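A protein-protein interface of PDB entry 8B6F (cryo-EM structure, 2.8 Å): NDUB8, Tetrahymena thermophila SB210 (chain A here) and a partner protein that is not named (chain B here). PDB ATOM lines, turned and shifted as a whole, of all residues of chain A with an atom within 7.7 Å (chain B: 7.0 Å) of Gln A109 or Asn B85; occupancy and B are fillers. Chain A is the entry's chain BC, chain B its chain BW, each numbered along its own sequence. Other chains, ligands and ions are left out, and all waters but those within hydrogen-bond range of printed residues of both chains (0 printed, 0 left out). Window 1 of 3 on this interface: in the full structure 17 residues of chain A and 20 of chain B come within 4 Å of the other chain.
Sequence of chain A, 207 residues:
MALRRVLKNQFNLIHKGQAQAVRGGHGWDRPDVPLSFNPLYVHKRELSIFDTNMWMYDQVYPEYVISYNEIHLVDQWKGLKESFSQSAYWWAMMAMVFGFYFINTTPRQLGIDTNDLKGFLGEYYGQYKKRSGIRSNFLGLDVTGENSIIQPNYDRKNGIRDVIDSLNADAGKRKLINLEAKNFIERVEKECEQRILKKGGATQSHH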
ATOM      1  N   THR A 106      18.572 -29.557  21.179  1.00  0.00           N
ATOM      2  CA  THR A 106      19.239 -28.343  20.741  1.00  0.00           C
ATOM      3  C   THR A 106      19.945 -27.691  21.920  1.00  0.00           C
ATOM      4  O   THR A 106      19.527 -27.865  23.068  1.00  0.00           O
ATOM      5  CB  THR A 106      18.239 -27.351  20.122  1.00  0.00           C
ATOM      6  OG1 THR A 106      18.884 -26.094  19.880  1.00  0.00           O
ATOM      7  CG2 THR A 106      17.051 -27.134  21.041  1.00  0.00           C
ATOM      8  N   PRO A 107      21.018 -26.940  21.671  1.00  0.00           N
ATOM      9  CA  PRO A 107      21.740 -26.311  22.783  1.00  0.00           C
ATOM     10  C   PRO A 107      20.858 -25.352  23.567  1.00  0.00           C
ATOM     11  O   PRO A 107      19.960 -24.709  23.022  1.00  0.00           O
ATOM     12  CB  PRO A 107      22.888 -25.570  22.089  1.00  0.00           C
ATOM     13  CG  PRO A 107      23.073 -26.275  20.801  1.00  0.00           C
ATOM     14  CD  PRO A 107      21.709 -26.731  20.386  1.00  0.00           C
ATOM     15  N   ARG A 108      21.130 -25.266  24.865  1.00  0.00           N
ATOM     16  CA  ARG A 108      20.410 -24.370  25.754  1.00  0.00           C
ATOM     17  C   ARG A 108      21.131 -23.031  25.870  1.00  0.00           C
ATOM     18  O   ARG A 108      22.300 -22.888  25.505  1.00  0.00           O
ATOM     19  CB  ARG A 108      20.256 -24.989  27.142  1.00  0.00           C
ATOM     20  CG  ARG A 108      19.512 -26.310  27.157  1.00  0.00           C
ATOM     21  CD  ARG A 108      19.287 -26.787  28.579  1.00  0.00           C
ATOM     22  NE  ARG A 108      20.540 -26.959  29.304  1.00  0.00           N
ATOM     23  CZ  ARG A 108      20.628 -27.209  30.603  1.00  0.00           C
ATOM     24  NH1 ARG A 108      19.550 -27.312  31.361  1.00  0.00           N
ATOM     25  NH2 ARG A 108      21.828 -27.364  31.154  1.00  0.00           N
ATOM     26  N   GLN A 109      20.410 -22.042  26.390  1.00  0.00           N
ATOM     27  CA  GLN A 109      20.960 -20.714  26.641  1.00  0.00           C
ATOM     28  C   GLN A 109      21.543 -20.695  28.050  1.00  0.00           C
ATOM     29  O   GLN A 109      20.799 -20.659  29.036  1.00  0.00           O
ATOM     30  CB  GLN A 109      19.880 -19.646  26.481  1.00  0.00           C
ATOM     31  CG  GLN A 109      19.139 -19.687  25.151  1.00  0.00           C
ATOM     32  CD  GLN A 109      20.035 -19.363  23.973  1.00  0.00           C
ATOM     33  OE1 GLN A 109      20.948 -20.119  23.645  1.00  0.00           O
ATOM     34  NE2 GLN A 109      19.782 -18.230  23.334  1.00  0.00           N
ATOM     35  N   LEU A 110      22.871 -20.721  28.149  1.00  0.00           N
ATOM     36  CA  LEU A 110      23.559 -20.752  29.431  1.00  0.00           C
ATOM     37  C   LEU A 110      24.677 -19.720  29.445  1.00  0.00           C
ATOM     38  O   LEU A 110      25.303 -19.446  28.419  1.00  0.00           O
ATOM     39  CB  LEU A 110      24.139 -22.143  29.722  1.00  0.00           C
ATOM     40  CG  LEU A 110      23.133 -23.290  29.858  1.00  0.00           C
ATOM     41  CD1 LEU A 110      23.861 -24.615  29.997  1.00  0.00           C
ATOM     42  CD2 LEU A 110      22.211 -23.066  31.042  1.00  0.00           C
ATOM     43  N   GLY A 111      24.922 -19.155  30.618  1.00  0.00           N
ATOM     44  CA  GLY A 111      25.970 -18.168  30.773  1.00  0.00           C
ATOM     45  C   GLY A 111      25.769 -17.375  32.050  1.00  0.00           C
ATOM     46  O   GLY A 111      24.883 -17.663  32.850  1.00  0.00           O
ATOM     47  N   THR A 114      22.856 -11.733  32.909  1.00  0.00           N
ATOM     48  CA  THR A 114      23.046 -10.455  32.238  1.00  0.00           C
ATOM     49  C   THR A 114      22.927  -9.276  33.196  1.00  0.00           C
ATOM     50  O   THR A 114      23.394  -8.181  32.870  1.00  0.00           O
ATOM     51  CB  THR A 114      22.033 -10.301  31.103  1.00  0.00           C
ATOM     52  OG1 THR A 114      20.701 -10.343  31.633  1.00  0.00           O
ATOM     53  CG2 THR A 114      22.203 -11.415  30.084  1.00  0.00           C
ATOM     54  N   ASP A 170      28.482 -14.854  25.216  1.00  0.00           N
ATOM     55  CA  ASP A 170      27.172 -15.483  25.351  1.00  0.00           C
ATOM     56  C   ASP A 170      26.177 -14.543  26.017  1.00  0.00           C
ATOM     57  O   ASP A 170      25.013 -14.469  25.609  1.00  0.00           O
ATOM     58  CB  ASP A 170      27.294 -16.786  26.141  1.00  0.00           C
ATOM     59  CG  ASP A 170      26.053 -17.655  26.032  1.00  0.00           C
ATOM     60  OD1 ASP A 170      24.934 -17.103  25.975  1.00  0.00           O
ATOM     61  OD2 ASP A 170      26.196 -18.895  25.999  1.00  0.00           O
ATOM     62  N   ALA A 171      26.613 -13.821  27.051  1.00  0.00           N
ATOM     63  CA  ALA A 171      25.728 -12.860  27.699  1.00  0.00           C
ATOM     64  C   ALA A 171      25.319 -11.759  26.731  1.00  0.00           C
ATOM     65  O   ALA A 171      24.147 -11.365  26.684  1.00  0.00           O
ATOM     66  CB  ALA A 171      26.410 -12.265  28.930  1.00  0.00           C
ATOM     67  N   GLY A 172      26.270 -11.248  25.951  1.00  0.00           N
ATOM     68  CA  GLY A 172      25.937 -10.249  24.950  1.00  0.00           C
ATOM     69  C   GLY A 172      24.959 -10.772  23.916  1.00  0.00           C
ATOM     70  O   GLY A 172      24.042 -10.061  23.499  1.00  0.00           O
ATOM     71  N   LYS A 173      25.142 -12.022  23.485  1.00  0.00           N
ATOM     72  CA  LYS A 173      24.228 -12.612  22.515  1.00  0.00           C
ATOM     73  C   LYS A 173      22.820 -12.737  23.085  1.00  0.00           C
ATOM     74  O   LYS A 173      21.837 -12.457  22.391  1.00  0.00           O
ATOM     75  CB  LYS A 173      24.751 -13.978  22.074  1.00  0.00           C
ATOM     76  CG  LYS A 173      23.972 -14.601  20.928  1.00  0.00           C
ATOM     77  CD  LYS A 173      24.617 -15.896  20.464  1.00  0.00           C
ATOM     78  CE  LYS A 173      23.902 -16.459  19.247  1.00  0.00           C
ATOM     79  NZ  LYS A 173      24.530 -17.718  18.763  1.00  0.00           N
ATOM     80  N   ARG A 174      22.701 -13.157  24.346  1.00  0.00           N
ATOM     81  CA  ARG A 174      21.380 -13.266  24.959  1.00  0.00           C
ATOM     82  C   ARG A 174      20.721 -11.898  25.095  1.00  0.00           C
ATOM     83  O   ARG A 174      19.514 -11.760  24.868  1.00  0.00           O
ATOM     84  CB  ARG A 174      21.481 -13.962  26.317  1.00  0.00           C
ATOM     85  CG  ARG A 174      21.700 -15.462  26.195  1.00  0.00           C
ATOM     86  CD  ARG A 174      21.675 -16.176  27.540  1.00  0.00           C
ATOM     87  NE  ARG A 174      22.942 -16.057  28.254  1.00  0.00           N
ATOM     88  CZ  ARG A 174      23.119 -15.410  29.399  1.00  0.00           C
ATOM     89  NH1 ARG A 174      22.117 -14.811  30.024  1.00  0.00           N
ATOM     90  NH2 ARG A 174      24.335 -15.361  29.932  1.00  0.00           N
ATOM     91  N   LYS A 175      21.490 -10.878  25.476  1.00  0.00           N
ATOM     92  CA  LYS A 175      20.942  -9.527  25.531  1.00  0.00           C
ATOM     93  C   LYS A 175      20.483  -9.070  24.152  1.00  0.00           C
ATOM     94  O   LYS A 175      19.434  -8.431  24.016  1.00  0.00           O
ATOM     95  CB  LYS A 175      21.976  -8.558  26.100  1.00  0.00           C
ATOM     96  CG  LYS A 175      22.319  -8.816  27.557  1.00  0.00           C
ATOM     97  CD  LYS A 175      23.425  -7.897  28.053  1.00  0.00           C
ATOM     98  CE  LYS A 175      22.969  -6.448  28.102  1.00  0.00           C
ATOM     99  NZ  LYS A 175      24.013  -5.562  28.688  1.00  0.00           N
ATOM    100  N   LEU A 176      21.262  -9.387  23.115  1.00  0.00           N
ATOM    101  CA  LEU A 176      20.866  -9.032  21.757  1.00  0.00           C
ATOM    102  C   LEU A 176      19.575  -9.734  21.363  1.00  0.00           C
ATOM    103  O   LEU A 176      18.708  -9.137  20.716  1.00  0.00           O
ATOM    104  CB  LEU A 176      21.987  -9.381  20.778  1.00  0.00           C
ATOM    105  CG  LEU A 176      21.736  -9.049  19.304  1.00  0.00           C
ATOM    106  CD1 LEU A 176      21.582  -7.549  19.102  1.00  0.00           C
ATOM    107  CD2 LEU A 176      22.860  -9.591  18.441  1.00  0.00           C
ATOM    108  N   ILE A 177      19.429 -11.003  21.745  1.00  0.00           N
ATOM    109  CA  ILE A 177      18.201 -11.733  21.442  1.00  0.00           C
ATOM    110  C   ILE A 177      17.008 -11.068  22.115  1.00  0.00           C
ATOM    111  O   ILE A 177      15.945 -10.904  21.506  1.00  0.00           O
ATOM    112  CB  ILE A 177      18.345 -13.208  21.862  1.00  0.00           C
ATOM    113  CG1 ILE A 177      19.356 -13.915  20.956  1.00  0.00           C
ATOM    114  CG2 ILE A 177      16.999 -13.921  21.824  1.00  0.00           C
ATOM    115  CD1 ILE A 177      19.796 -15.268  21.465  1.00  0.00           C
ATOM    116  N   ASN A 178      17.156 -10.686  23.383  1.00  0.00           N
ATOM    117  CA  ASN A 178      16.068 -10.003  24.073  1.00  0.00           C
ATOM    118  C   ASN A 178      15.725  -8.685  23.390  1.00  0.00           C
ATOM    119  O   ASN A 178      14.547  -8.357  23.215  1.00  0.00           O
ATOM    120  CB  ASN A 178      16.444  -9.761  25.534  1.00  0.00           C
ATOM    121  CG  ASN A 178      16.566 -11.047  26.326  1.00  0.00           C
ATOM    122  OD1 ASN A 178      15.868 -12.023  26.060  1.00  0.00           O
ATOM    123  ND2 ASN A 178      17.461 -11.053  27.305  1.00  0.00           N
ATOM    124  N   LEU A 179      16.743  -7.915  22.998  1.00  0.00           N
ATOM    125  CA  LEU A 179      16.490  -6.645  22.326  1.00  0.00           C
ATOM    126  C   LEU A 179      15.776  -6.857  20.996  1.00  0.00           C
ATOM    127  O   LEU A 179      14.866  -6.098  20.643  1.00  0.00           O
ATOM    128  CB  LEU A 179      17.806  -5.895  22.114  1.00  0.00           C
ATOM    129  CG  LEU A 179      17.706  -4.546  21.399  1.00  0.00           C
ATOM    130  CD1 LEU A 179      16.794  -3.591  22.150  1.00  0.00           C
ATOM    131  CD2 LEU A 179      19.086  -3.939  21.230  1.00  0.00           C
ATOM    132  N   TRP B  79      12.533 -11.974  35.368  1.00  0.00           N
ATOM    133  CA  TRP B  79      13.981 -12.132  35.456  1.00  0.00           C
ATOM    134  C   TRP B  79      14.430 -13.439  34.814  1.00  0.00           C
ATOM    135  O   TRP B  79      15.343 -13.453  33.981  1.00  0.00           O
ATOM    136  CB  TRP B  79      14.406 -12.070  36.924  1.00  0.00           C
ATOM    137  CG  TRP B  79      15.841 -12.404  37.180  1.00  0.00           C
ATOM    138  CD1 TRP B  79      16.890 -12.259  36.321  1.00  0.00           C
ATOM    139  CD2 TRP B  79      16.385 -12.943  38.390  1.00  0.00           C
ATOM    140  NE1 TRP B  79      18.053 -12.675  36.921  1.00  0.00           N
ATOM    141  CE2 TRP B  79      17.769 -13.099  38.193  1.00  0.00           C
ATOM    142  CE3 TRP B  79      15.832 -13.308  39.622  1.00  0.00           C
ATOM    143  CZ2 TRP B  79      18.611 -13.605  39.181  1.00  0.00           C
ATOM    144  CZ3 TRP B  79      16.669 -13.810  40.602  1.00  0.00           C
ATOM    145  CH2 TRP B  79      18.044 -13.954  40.377  1.00  0.00           C
ATOM    146  N   GLN B  80      13.802 -14.552  35.194  1.00  0.00           N
ATOM    147  CA  GLN B  80      14.218 -15.847  34.666  1.00  0.00           C
ATOM    148  C   GLN B  80      13.906 -15.969  33.180  1.00  0.00           C
ATOM    149  O   GLN B  80      14.694 -16.544  32.421  1.00  0.00           O
ATOM    150  CB  GLN B  80      13.550 -16.973  35.452  1.00  0.00           C
ATOM    151  CG  GLN B  80      13.850 -16.940  36.940  1.00  0.00           C
ATOM    152  CD  GLN B  80      15.331 -17.042  37.244  1.00  0.00           C
ATOM    153  OE1 GLN B  80      16.135 -17.377  36.377  1.00  0.00           O
ATOM    154  NE2 GLN B  80      15.700 -16.753  38.486  1.00  0.00           N
ATOM    155  N   THR B  81      12.759 -15.444  32.744  1.00  0.00           N
ATOM    156  CA  THR B  81      12.420 -15.500  31.325  1.00  0.00           C
ATOM    157  C   THR B  81      13.441 -14.744  30.486  1.00  0.00           C
ATOM    158  O   THR B  81      13.849 -15.216  29.418  1.00  0.00           O
ATOM    159  CB  THR B  81      11.019 -14.937  31.096  1.00  0.00           C
ATOM    160  OG1 THR B  81      10.062 -15.714  31.824  1.00  0.00           O
ATOM    161  CG2 THR B  81      10.664 -14.964  29.617  1.00  0.00           C
ATOM    162  N   TYR B  82      13.862 -13.564  30.943  1.00  0.00           N
ATOM    163  CA  TYR B  82      14.855 -12.802  30.196  1.00  0.00           C
ATOM    164  C   TYR B  82      16.237 -13.429  30.300  1.00  0.00           C
ATOM    165  O   TYR B  82      17.048 -13.287  29.380  1.00  0.00           O
ATOM    166  CB  TYR B  82      14.892 -11.355  30.690  1.00  0.00           C
ATOM    167  CG  TYR B  82      13.590 -10.607  30.502  1.00  0.00           C
ATOM    168  CD1 TYR B  82      12.725 -10.923  29.463  1.00  0.00           C
ATOM    169  CD2 TYR B  82      13.224  -9.588  31.369  1.00  0.00           C
ATOM    170  CE1 TYR B  82      11.537 -10.247  29.293  1.00  0.00           C
ATOM    171  CE2 TYR B  82      12.037  -8.903  31.207  1.00  0.00           C
ATOM    172  CZ  TYR B  82      11.197  -9.240  30.165  1.00  0.00           C
ATOM    173  OH  TYR B  82      10.012  -8.564  29.996  1.00  0.00           O
ATOM    174  N   GLU B  83      16.528 -14.120  31.402  1.00  0.00           N
ATOM    175  CA  GLU B  83      17.833 -14.759  31.533  1.00  0.00           C
ATOM    176  C   GLU B  83      17.984 -15.930  30.568  1.00  0.00           C
ATOM    177  O   GLU B  83      19.029 -16.071  29.923  1.00  0.00           O
ATOM    178  CB  GLU B  83      18.040 -15.224  32.974  1.00  0.00           C
ATOM    179  CG  GLU B  83      18.423 -14.110  33.935  1.00  0.00           C
ATOM    180  CD  GLU B  83      19.800 -13.543  33.649  1.00  0.00           C
ATOM    181  OE1 GLU B  83      20.503 -14.096  32.779  1.00  0.00           O
ATOM    182  OE2 GLU B  83      20.178 -12.542  34.292  1.00  0.00           O
ATOM    183  N   ASN B  84      16.966 -16.782  30.457  1.00  0.00           N
ATOM    184  CA  ASN B  84      17.049 -17.955  29.595  1.00  0.00           C
ATOM    185  C   ASN B  84      16.465 -17.723  28.205  1.00  0.00           C
ATOM    186  O   ASN B  84      16.501 -18.641  27.379  1.00  0.00           O
ATOM    187  CB  ASN B  84      16.350 -19.155  30.247  1.00  0.00           C
ATOM    188  CG  ASN B  84      14.874 -18.926  30.471  1.00  0.00           C
ATOM    189  OD1 ASN B  84      14.319 -17.913  30.050  1.00  0.00           O
ATOM    190  ND2 ASN B  84      14.224 -19.876  31.129  1.00  0.00           N
ATOM    191  N   ASN B  85      15.943 -16.529  27.921  1.00  0.00           N
ATOM    192  CA  ASN B  85      15.353 -16.228  26.616  1.00  0.00           C
ATOM    193  C   ASN B  85      14.257 -17.227  26.257  1.00  0.00           C
ATOM    194  O   ASN B  85      14.097 -17.612  25.097  1.00  0.00           O
ATOM    195  CB  ASN B  85      16.423 -16.196  25.526  1.00  0.00           C
ATOM    196  CG  ASN B  85      17.402 -15.063  25.710  1.00  0.00           C
ATOM    197  OD1 ASN B  85      17.413 -14.398  26.742  1.00  0.00           O
ATOM    198  ND2 ASN B  85      18.235 -14.838  24.706  1.00  0.00           N
ATOM    199  N   SER B  86      13.482 -17.645  27.259  1.00  0.00           N
ATOM    200  CA  SER B  86      12.464 -18.663  27.022  1.00  0.00           C
ATOM    201  C   SER B  86      11.271 -18.107  26.253  1.00  0.00           C
ATOM    202  O   SER B  86      10.588 -18.860  25.551  1.00  0.00           O
ATOM    203  CB  SER B  86      12.004 -19.270  28.347  1.00  0.00           C
ATOM    204  OG  SER B  86      11.398 -18.295  29.178  1.00  0.00           O
ATOM    205  N   HIS B  87      10.994 -16.807  26.374  1.00  0.00           N
ATOM    206  CA  HIS B  87       9.839 -16.248  25.679  1.00  0.00           C
ATOM    207  C   HIS B  87      10.031 -16.281  24.168  1.00  0.00           C
ATOM    208  O   HIS B  87       9.047 -16.338  23.422  1.00  0.00           O
ATOM    209  CB  HIS B  87       9.563 -14.821  26.158  1.00  0.00           C
ATOM    210  CG  HIS B  87      10.675 -13.856  25.882  1.00  0.00           C
ATOM    211  ND1 HIS B  87      11.836 -13.823  26.624  1.00  0.00           N
ATOM    212  CD2 HIS B  87      10.792 -12.874  24.959  1.00  0.00           C
ATOM    213  CE1 HIS B  87      12.625 -12.870  26.160  1.00  0.00           C
ATOM    214  NE2 HIS B  87      12.014 -12.278  25.151  1.00  0.00           N
ATOM    215  N   VAL B  88      11.276 -16.249  23.702  1.00  0.00           N
ATOM    216  CA  VAL B  88      11.563 -16.357  22.276  1.00  0.00           C
ATOM    217  C   VAL B  88      11.730 -17.812  21.862  1.00  0.00           C
ATOM    218  O   VAL B  88      11.287 -18.211  20.782  1.00  0.00           O
ATOM    219  CB  VAL B  88      12.815 -15.533  21.921  1.00  0.00           C
ATOM    220  CG1 VAL B  88      13.033 -15.518  20.419  1.00  0.00           C
ATOM    221  CG2 VAL B  88      12.698 -14.119  22.457  1.00  0.00           C
ATOM    222  N   THR B  89      12.373 -18.618  22.707  1.00  0.00           N
ATOM    223  CA  THR B  89      12.567 -20.027  22.386  1.00  0.00           C
ATOM    224  C   THR B  89      11.233 -20.751  22.267  1.00  0.00           C
ATOM    225  O   THR B  89      11.050 -21.586  21.373  1.00  0.00           O
ATOM    226  CB  THR B  89      13.441 -20.688  23.452  1.00  0.00           C
ATOM    227  OG1 THR B  89      14.693 -19.996  23.546  1.00  0.00           O
ATOM    228  CG2 THR B  89      13.698 -22.148  23.110  1.00  0.00           C
ATOM    229  N   ASN B  90      10.292 -20.452  23.162  1.00  0.00           N
ATOM    230  CA  ASN B  90       8.978 -21.081  23.088  1.00  0.00           C
ATOM    231  C   ASN B  90       8.235 -20.666  21.825  1.00  0.00           C
ATOM    232  O   ASN B  90       7.562 -21.490  21.198  1.00  0.00           O
ATOM    233  CB  ASN B  90       8.159 -20.738  24.331  1.00  0.00           C
ATOM    234  CG  ASN B  90       8.604 -21.516  25.553  1.00  0.00           C
ATOM    235  OD1 ASN B  90       9.709 -22.050  25.592  1.00  0.00           O
ATOM    236  ND2 ASN B  90       7.741 -21.583  26.558  1.00  0.00           N
ATOM    237  N   SER B 105      13.857 -12.915  16.473  1.00  0.00           N
ATOM    238  CA  SER B 105      15.259 -12.622  16.757  1.00  0.00           C
ATOM    239  C   SER B 105      16.093 -13.464  15.796  1.00  0.00           C
ATOM    240  O   SER B 105      16.246 -14.672  16.002  1.00  0.00           O
ATOM    241  CB  SER B 105      15.606 -12.922  18.209  1.00  0.00           C
ATOM    242  OG  SER B 105      15.407 -14.295  18.501  1.00  0.00           O
ATOM    243  N   TYR B 108      18.894 -15.851  17.253  1.00  0.00           N
ATOM    244  CA  TYR B 108      18.518 -17.195  17.677  1.00  0.00           C
ATOM    245  C   TYR B 108      17.938 -18.018  16.535  1.00  0.00           C
ATOM    246  O   TYR B 108      18.125 -19.239  16.499  1.00  0.00           O
ATOM    247  CB  TYR B 108      17.512 -17.122  18.826  1.00  0.00           C
ATOM    248  CG  TYR B 108      17.144 -18.475  19.386  1.00  0.00           C
ATOM    249  CD1 TYR B 108      17.967 -19.113  20.304  1.00  0.00           C
ATOM    250  CD2 TYR B 108      15.978 -19.114  18.996  1.00  0.00           C
ATOM    251  CE1 TYR B 108      17.638 -20.350  20.817  1.00  0.00           C
ATOM    252  CE2 TYR B 108      15.639 -20.352  19.503  1.00  0.00           C
ATOM    253  CZ  TYR B 108      16.474 -20.965  20.413  1.00  0.00           C
ATOM    254  OH  TYR B 108      16.142 -22.196  20.922  1.00  0.00           O
ATOM    255  N   SER B 111      20.361 -20.191  14.221  1.00  0.00           N
ATOM    256  CA  SER B 111      20.980 -21.375  14.797  1.00  0.00           C
ATOM    257  C   SER B 111      19.980 -22.358  15.388  1.00  0.00           C
ATOM    258  O   SER B 111      20.361 -23.496  15.683  1.00  0.00           O
ATOM    259  CB  SER B 111      21.988 -20.969  15.884  1.00  0.00           C
ATOM    260  OG  SER B 111      21.354 -20.238  16.920  1.00  0.00           O
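The guanidinium group (NH1) of Arg A174 lies within salt-bridge range of the side-chain carboxylate (OE1) of Glu B83. N of Thr A114 lies within hydrogen-bond range of OE2 of Glu B83, at 3.1 Å. ND2 of Asn B85 sits at hydrogen-bond distance from O of Arg A174, 3.3 Å away. The side-chain amide nitrogen (ND2) of Asn A178 is in hydrogen-bond range of the backbone carbonyl oxygen (O) of Tyr B82, at 3.1 Å. OD1 of Asn A178 sits close to OD1 of Asn B85, at 2.9 Å.
The side-chain amide oxygen (OD1) of Asn B84 lies close to the backbone carbonyl oxygen (O) of Gln B80, at 2.8 Å. The side-chain hydroxyl (OG) of Ser B111 sits at hydrogen-bond distance from the backbone carbonyl oxygen (O) of Tyr B108, 3.4 Å away. O of Asn B85 is in hydrogen-bond range of OG1 of Thr B89 (2.9 Å). The side-chain carboxylate of Asp A170 is in salt-bridge range of the guanidinium group of Arg A174, at 3.2 Å. The side-chain amide oxygen of Asn B84 sits at hydrogen-bond distance from the backbone NH of Ser B86, at 2.9 Å. OD1 of Asn B85 lies close to O of Tyr B82 (2.9 Å).
Among the printed residues, merely in contact across the chains: Ile A177 with Asn B85 (3.3 Å), Asn A178 with His B87 (3.4 Å), Gln A109 with Asn B84 (3.6 Å), Gln A109 with Tyr B108 (3.6 Å), Ile A177 with Ser B105 (3.7 Å), Ile A177 with Tyr B108 (3.95 Å) and Gln A109 with Asn B85 (3.97 Å).
Of chain B, only Asn B84 (3.6 Å), Asn B85 (3.97 Å) and Tyr B108 (3.6 Å) come within 4 Å of Gln A109. Printed residues of chain B within 4 Å of Ile A177: Asn B85, Ser B105 and Tyr B108. Of the printed residues of chain A, Tyr B82 touches Asn A178 (3.1 Å). Of chain A, only Gln A109 (3.97 Å), Arg A174 (3.3 Å), Ile A177 (3.3 Å) and Asn A178 (2.9 Å) come within 4 Å of Asn B85. Ser B86 touches none of the printed residues of chain A. Of the printed residues of chain A, His B87 touches Asn A178 (3.4 Å). The nearest residue of chain B that does not touch Gln A109 is Thr B89 (4.7 Å). The nearest printed residue of chain A that does not touch Tyr B108 is Thr A106 (4.9 Å).
Of the 17 printed residues of chain A, 5 touch a printed residue of chain B. Hydrophobic or aromatic side chains of chain A within 4 Å of the printed part of chain B: Ile A177. Among the printed residues, Asp or Glu carboxylates within 4 Å of a Lys or Arg side-chain nitrogen of the other chain: Arg A174 with Glu B83.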
